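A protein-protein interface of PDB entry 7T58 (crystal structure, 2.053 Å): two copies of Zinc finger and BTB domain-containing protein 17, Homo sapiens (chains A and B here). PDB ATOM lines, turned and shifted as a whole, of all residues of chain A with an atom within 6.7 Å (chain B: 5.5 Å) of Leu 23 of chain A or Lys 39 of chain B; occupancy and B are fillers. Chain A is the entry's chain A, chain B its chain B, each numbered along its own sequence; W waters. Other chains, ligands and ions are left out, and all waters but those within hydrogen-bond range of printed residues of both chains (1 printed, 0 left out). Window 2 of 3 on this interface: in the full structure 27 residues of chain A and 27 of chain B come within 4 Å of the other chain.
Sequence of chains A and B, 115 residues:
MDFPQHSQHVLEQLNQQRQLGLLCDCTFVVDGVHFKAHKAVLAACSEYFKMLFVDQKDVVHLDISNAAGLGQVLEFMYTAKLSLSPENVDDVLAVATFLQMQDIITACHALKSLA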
ATOM      1  N   GLN A  17     -28.457  13.192  16.967  1.00  0.00           N
ATOM      2  CA  GLN A  17     -27.588  13.631  15.879  1.00  0.00           C
ATOM      3  C   GLN A  17     -28.097  14.923  15.255  1.00  0.00           C
ATOM      4  O   GLN A  17     -27.313  15.832  14.957  1.00  0.00           O
ATOM      5  CB  GLN A  17     -27.488  12.547  14.804  1.00  0.00           C
ATOM      6  CG  GLN A  17     -26.885  11.233  15.254  1.00  0.00           C
ATOM      7  CD  GLN A  17     -26.973  10.175  14.173  1.00  0.00           C
ATOM      8  OE1 GLN A  17     -27.263  10.481  13.015  1.00  0.00           O
ATOM      9  NE2 GLN A  17     -26.734   8.923  14.546  1.00  0.00           N
ATOM     10  N   LEU A  20     -27.552  18.091  17.290  1.00  0.00           N
ATOM     11  CA  LEU A  20     -26.153  18.489  17.343  1.00  0.00           C
ATOM     12  C   LEU A  20     -25.564  18.743  15.959  1.00  0.00           C
ATOM     13  O   LEU A  20     -24.363  19.003  15.844  1.00  0.00           O
ATOM     14  CB  LEU A  20     -25.336  17.424  18.078  1.00  0.00           C
ATOM     15  CG  LEU A  20     -25.887  16.998  19.442  1.00  0.00           C
ATOM     16  CD1 LEU A  20     -25.057  15.873  20.042  1.00  0.00           C
ATOM     17  CD2 LEU A  20     -25.956  18.186  20.394  1.00  0.00           C
ATOM     18  N   GLY A  21     -26.380  18.684  14.908  1.00  0.00           N
ATOM     19  CA  GLY A  21     -25.881  18.916  13.567  1.00  0.00           C
ATOM     20  C   GLY A  21     -25.005  17.816  13.015  1.00  0.00           C
ATOM     21  O   GLY A  21     -24.266  18.048  12.055  1.00  0.00           O
ATOM     22  N   LEU A  22     -25.074  16.616  13.589  1.00  0.00           N
ATOM     23  CA  LEU A  22     -24.210  15.511  13.195  1.00  0.00           C
ATOM     24  C   LEU A  22     -24.848  14.720  12.060  1.00  0.00           C
ATOM     25  O   LEU A  22     -26.045  14.416  12.102  1.00  0.00           O
ATOM     26  CB  LEU A  22     -23.946  14.591  14.386  1.00  0.00           C
ATOM     27  CG  LEU A  22     -23.457  15.255  15.673  1.00  0.00           C
ATOM     28  CD1 LEU A  22     -23.758  14.365  16.867  1.00  0.00           C
ATOM     29  CD2 LEU A  22     -21.972  15.556  15.588  1.00  0.00           C
ATOM     30  N   LEU A  23     -24.041  14.384  11.052  1.00  0.00           N
ATOM     31  CA  LEU A  23     -24.447  13.531   9.936  1.00  0.00           C
ATOM     32  C   LEU A  23     -25.680  14.058   9.207  1.00  0.00           C
ATOM     33  O   LEU A  23     -26.375  13.295   8.530  1.00  0.00           O
ATOM     34  CB  LEU A  23     -24.685  12.088  10.399  1.00  0.00           C
ATOM     35  CG  LEU A  23     -23.445  11.298  10.820  1.00  0.00           C
ATOM     36  CD1 LEU A  23     -23.841   9.950  11.397  1.00  0.00           C
ATOM     37  CD2 LEU A  23     -22.497  11.119   9.644  1.00  0.00           C
ATOM     38  N   CYS A  24     -25.974  15.350   9.335  1.00  0.00           N
ATOM     39  CA  CYS A  24     -27.039  15.964   8.557  1.00  0.00           C
ATOM     40  C   CYS A  24     -26.507  16.311   7.174  1.00  0.00           C
ATOM     41  O   CYS A  24     -25.457  16.949   7.050  1.00  0.00           O
ATOM     42  CB  CYS A  24     -27.567  17.216   9.258  1.00  0.00           C
ATOM     43  SG  CYS A  24     -28.387  16.895  10.834  1.00  0.00           S
ATOM     44  N   ASP A  25     -27.222  15.883   6.134  1.00  0.00           N
ATOM     45  CA  ASP A  25     -26.749  16.054   4.766  1.00  0.00           C
ATOM     46  C   ASP A  25     -27.685  16.896   3.909  1.00  0.00           C
ATOM     47  O   ASP A  25     -27.464  17.003   2.697  1.00  0.00           O
ATOM     48  CB  ASP A  25     -26.512  14.691   4.108  1.00  0.00           C
ATOM     49  CG  ASP A  25     -27.712  13.773   4.216  1.00  0.00           C
ATOM     50  OD1 ASP A  25     -28.600  14.044   5.052  1.00  0.00           O
ATOM     51  OD2 ASP A  25     -27.762  12.772   3.467  1.00  0.00           O
ATOM     52  N   CYS A  26     -28.716  17.500   4.493  1.00  0.00           N
ATOM     53  CA  CYS A  26     -29.516  18.475   3.770  1.00  0.00           C
ATOM     54  C   CYS A  26     -29.909  19.599   4.715  1.00  0.00           C
ATOM     55  O   CYS A  26     -30.209  19.373   5.890  1.00  0.00           O
ATOM     56  CB  CYS A  26     -30.766  17.849   3.136  1.00  0.00           C
ATOM     57  SG  CYS A  26     -32.054  17.367   4.296  1.00  0.00           S
ATOM     58  N   ALA A  37     -31.239  18.416   8.634  1.00  0.00           N
ATOM     59  CA  ALA A  37     -31.800  17.097   8.901  1.00  0.00           C
ATOM     60  C   ALA A  37     -31.118  16.075   8.001  1.00  0.00           C
ATOM     61  O   ALA A  37     -30.235  16.407   7.206  1.00  0.00           O
ATOM     62  CB  ALA A  37     -33.318  17.095   8.696  1.00  0.00           C
ATOM     63  N   HIS A  38     -31.539  14.818   8.137  1.00  0.00           N
ATOM     64  CA  HIS A  38     -31.041  13.730   7.307  1.00  0.00           C
ATOM     65  C   HIS A  38     -31.938  13.562   6.087  1.00  0.00           C
ATOM     66  O   HIS A  38     -33.166  13.517   6.219  1.00  0.00           O
ATOM     67  CB  HIS A  38     -30.998  12.413   8.087  1.00  0.00           C
ATOM     68  CG  HIS A  38     -30.335  12.512   9.424  1.00  0.00           C
ATOM     69  ND1 HIS A  38     -30.963  13.046  10.528  1.00  0.00           N
ATOM     70  CD2 HIS A  38     -29.109  12.119   9.841  1.00  0.00           C
ATOM     71  CE1 HIS A  38     -30.147  12.990  11.566  1.00  0.00           C
ATOM     72  NE2 HIS A  38     -29.014  12.434  11.175  1.00  0.00           N
ATOM     73  N   LYS A  39     -31.324  13.461   4.902  1.00  0.00           N
ATOM     74  CA  LYS A  39     -32.081  13.118   3.700  1.00  0.00           C
ATOM     75  C   LYS A  39     -32.871  11.830   3.901  1.00  0.00           C
ATOM     76  O   LYS A  39     -34.046  11.738   3.530  1.00  0.00           O
ATOM     77  CB  LYS A  39     -31.144  12.961   2.499  1.00  0.00           C
ATOM     78  CG  LYS A  39     -30.500  14.230   1.973  1.00  0.00           C
ATOM     79  CD  LYS A  39     -29.688  13.892   0.726  1.00  0.00           C
ATOM     80  CE  LYS A  39     -28.571  14.889   0.473  1.00  0.00           C
ATOM     81  NZ  LYS A  39     -29.072  16.178  -0.071  1.00  0.00           N
ATOM     82  N   ASP B  25     -24.699   6.049   2.353  1.00  0.00           N
ATOM     83  CA  ASP B  25     -23.432   6.759   2.255  1.00  0.00           C
ATOM     84  C   ASP B  25     -22.267   5.969   2.844  1.00  0.00           C
ATOM     85  O   ASP B  25     -21.190   6.533   3.067  1.00  0.00           O
ATOM     86  CB  ASP B  25     -23.542   8.128   2.930  1.00  0.00           C
ATOM     87  CG  ASP B  25     -24.066   8.039   4.353  1.00  0.00           C
ATOM     88  OD1 ASP B  25     -24.383   6.919   4.806  1.00  0.00           O
ATOM     89  OD2 ASP B  25     -24.162   9.091   5.018  1.00  0.00           O
ATOM     90  N   CYS B  26     -22.456   4.678   3.096  1.00  0.00           N
ATOM     91  CA  CYS B  26     -21.391   3.833   3.615  1.00  0.00           C
ATOM     92  C   CYS B  26     -21.428   2.498   2.890  1.00  0.00           C
ATOM     93  O   CYS B  26     -22.487   1.869   2.800  1.00  0.00           O
ATOM     94  CB  CYS B  26     -21.529   3.625   5.128  1.00  0.00           C
ATOM     95  SG  CYS B  26     -20.176   2.684   5.860  1.00  0.00           S
ATOM     96  N   ALA B  37     -25.174   0.800   3.660  1.00  0.00           N
ATOM     97  CA  ALA B  37     -25.962   1.209   4.817  1.00  0.00           C
ATOM     98  C   ALA B  37     -25.863   2.721   4.973  1.00  0.00           C
ATOM     99  O   ALA B  37     -25.115   3.392   4.256  1.00  0.00           O
ATOM    100  CB  ALA B  37     -25.499   0.492   6.089  1.00  0.00           C
ATOM    101  N   HIS B  38     -26.628   3.252   5.927  1.00  0.00           N
ATOM    102  CA  HIS B  38     -26.593   4.664   6.283  1.00  0.00           C
ATOM    103  C   HIS B  38     -25.625   4.862   7.440  1.00  0.00           C
ATOM    104  O   HIS B  38     -25.698   4.142   8.443  1.00  0.00           O
ATOM    105  CB  HIS B  38     -27.976   5.181   6.693  1.00  0.00           C
ATOM    106  CG  HIS B  38     -29.063   4.907   5.701  1.00  0.00           C
ATOM    107  ND1 HIS B  38     -29.773   3.725   5.680  1.00  0.00           N
ATOM    108  CD2 HIS B  38     -29.585   5.676   4.715  1.00  0.00           C
ATOM    109  CE1 HIS B  38     -30.675   3.772   4.715  1.00  0.00           C
ATOM    110  NE2 HIS B  38     -30.580   4.945   4.113  1.00  0.00           N
ATOM    111  N   LYS B  39     -24.729   5.843   7.307  1.00  0.00           N
ATOM    112  CA  LYS B  39     -23.845   6.187   8.416  1.00  0.00           C
ATOM    113  C   LYS B  39     -24.644   6.537   9.663  1.00  0.00           C
ATOM    114  O   LYS B  39     -24.264   6.169  10.780  1.00  0.00           O
ATOM    115  CB  LYS B  39     -22.932   7.352   8.027  1.00  0.00           C
ATOM    116  CG  LYS B  39     -21.877   7.010   6.990  1.00  0.00           C
ATOM    117  CD  LYS B  39     -20.949   8.192   6.745  1.00  0.00           C
ATOM    118  CE  LYS B  39     -19.862   7.846   5.736  1.00  0.00           C
ATOM    119  NZ  LYS B  39     -18.871   8.947   5.567  1.00  0.00           N
ATOM    120  N   ALA B  40     -25.765   7.241   9.487  1.00  0.00           N
ATOM    121  CA  ALA B  40     -26.560   7.671  10.632  1.00  0.00           C
ATOM    122  C   ALA B  40     -27.136   6.482  11.390  1.00  0.00           C
ATOM    123  O   ALA B  40     -27.206   6.500  12.624  1.00  0.00           O
ATOM    124  CB  ALA B  40     -27.677   8.607  10.168  1.00  0.00           C
ATOM    125  N   VAL B  41     -27.556   5.440  10.672  1.00  0.00           N
ATOM    126  CA  VAL B  41     -28.125   4.269  11.332  1.00  0.00           C
ATOM    127  C   VAL B  41     -27.028   3.417  11.956  1.00  0.00           C
ATOM    128  O   VAL B  41     -27.178   2.920  13.079  1.00  0.00           O
ATOM    129  CB  VAL B  41     -28.982   3.463  10.339  1.00  0.00           C
ATOM    130  CG1 VAL B  41     -29.370   2.117  10.930  1.00  0.00           C
ATOM    131  CG2 VAL B  41     -30.227   4.242   9.980  1.00  0.00           C
ATOM    132  N   LEU B  42     -25.911   3.241  11.248  1.00  0.00           N
ATOM    133  CA  LEU B  42     -24.780   2.508  11.809  1.00  0.00           C
ATOM    134  C   LEU B  42     -24.317   3.138  13.114  1.00  0.00           C
ATOM    135  O   LEU B  42     -24.128   2.446  14.120  1.00  0.00           O
ATOM    136  CB  LEU B  42     -23.631   2.461  10.799  1.00  0.00           C
ATOM    137  CG  LEU B  42     -23.879   1.702   9.493  1.00  0.00           C
ATOM    138  CD1 LEU B  42     -22.678   1.803   8.575  1.00  0.00           C
ATOM    139  CD2 LEU B  42     -24.215   0.252   9.778  1.00  0.00           C
ATOM    140  N   ALA B  43     -24.141   4.462  13.118  1.00  0.00           N
ATOM    141  CA  ALA B  43     -23.709   5.146  14.331  1.00  0.00           C
ATOM    142  C   ALA B  43     -24.765   5.068  15.423  1.00  0.00           C
ATOM    143  O   ALA B  43     -24.432   5.124  16.613  1.00  0.00           O
ATOM    144  CB  ALA B  43     -23.372   6.604  14.017  1.00  0.00           C
ATOM    145  N   ALA B  44     -26.038   4.935  15.044  1.00  0.00           N
ATOM    146  CA  ALA B  44     -27.097   4.855  16.045  1.00  0.00           C
ATOM    147  C   ALA B  44     -27.091   3.515  16.767  1.00  0.00           C
ATOM    148  O   ALA B  44     -27.504   3.438  17.930  1.00  0.00           O
ATOM    149  CB  ALA B  44     -28.457   5.095  15.391  1.00  0.00           C
ATOM    150  N   PHE B  53     -17.987   7.792  12.877  1.00  0.00           N
ATOM    151  CA  PHE B  53     -18.739   8.778  12.111  1.00  0.00           C
ATOM    152  C   PHE B  53     -19.168   9.992  12.923  1.00  0.00           C
ATOM    153  O   PHE B  53     -19.317  11.080  12.350  1.00  0.00           O
ATOM    154  CB  PHE B  53     -19.982   8.130  11.490  1.00  0.00           C
ATOM    155  CG  PHE B  53     -19.671   7.009  10.539  1.00  0.00           C
ATOM    156  CD1 PHE B  53     -18.649   7.134   9.612  1.00  0.00           C
ATOM    157  CD2 PHE B  53     -20.394   5.826  10.576  1.00  0.00           C
ATOM    158  CE1 PHE B  53     -18.355   6.103   8.735  1.00  0.00           C
ATOM    159  CE2 PHE B  53     -20.103   4.789   9.701  1.00  0.00           C
ATOM    160  CZ  PHE B  53     -19.083   4.930   8.781  1.00  0.00           C
ATOM    161  N   VAL B  54     -19.384   9.845  14.226  1.00  0.00           N
ATOM    162  CA  VAL B  54     -19.895  10.924  15.062  1.00  0.00           C
ATOM    163  C   VAL B  54     -18.798  11.517  15.939  1.00  0.00           C
ATOM    164  O   VAL B  54     -18.538  12.723  15.895  1.00  0.00           O
ATOM    165  CB  VAL B  54     -21.091  10.443  15.912  1.00  0.00           C
ATOM    166  CG1 VAL B  54     -21.477  11.508  16.920  1.00  0.00           C
ATOM    167  CG2 VAL B  54     -22.270  10.092  15.011  1.00  0.00           C
HETATM  168  O   HOH W   1     -25.706   8.188  17.047  1.00  0.00           O
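5 positions are printed for both chains.
Of the 11 printed residues of chain A, 4 touch a printed residue of chain B.
Printed residues of chain A that touch a printed residue of chain B: Gln 17, Leu 22, Leu 23 and His 38.
Hydrophobic or aromatic side chains of chain A within 4 Å of the printed part of chain B: Leu 22, Leu 23 and His 38.
Along chain A the printed residues that touch a printed residue of chain B span positions 17 to 38.
Hydrophobic or aromatic side chains of chain B that line the printed part of chain A: Ala 40 and Val 54.
Among the printed residues, no Asp or Glu carboxylate lies within 4 Å of a Lys or Arg side-chain nitrogen of the other chain.
The side-chain carboxylate (OD1) of Asp 25 of chain B is in hydrogen-bond range of the backbone NH (N) of Lys 39 of chain B, at 2.7 Å.
SG of Cys 24 of chain A lies within hydrogen-bond range of O of Leu 22 of chain A (3.6 Å).
O of Gln 17 of chain A sits at hydrogen-bond distance from N of Leu 22 of chain A (2.7 Å).
NE2 of His 38 of chain A is in hydrogen-bond range of OE1 of Gln 17 of chain A (3.2 Å).
Among the printed residues, merely in contact across the chains: Leu 22 of chain A with Val 54 of chain B (3.7 Å), Leu 23 of chain A with Lys 39 of chain B (3.9 Å), Leu 23 of chain A with Ala 40 of chain B (3.6 Å), Leu 23 of chain A with Val 54 of chain B (3.9 Å) and His 38 of chain A with Ala 40 of chain B (3.8 Å).
Water W1 lies within hydrogen-bond range of NE2 of Gln 17 of chain A (2.8 Å) and O of Ala 43 of chain B (3.3 Å).
O of Ala 40 of chain B is in hydrogen-bond range of NE2 of Gln 17 of chain A (3.1 Å).
Lys 39 of chain B touches one residue of chain A.
Printed residues of chain B within 4 Å of Gln 17 of chain A: Ala 40 (3.1 Å).
Printed residues of chain B within 4 Å of His 38 of chain A: Ala 40.
Printed residues of chain B within 4 Å of Leu 22 of chain A: Val 54.
Printed residues of chain A within 4 Å of Val 54 of chain B: Leu 22 (3.7 Å) and Leu 23 (3.9 Å).
Phe 53 of chain B touches none of the printed residues of chain A.
The nearest residue of chain A that does not touch Lys 39 of chain B is Gln 17 of chain A (5.3 Å).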
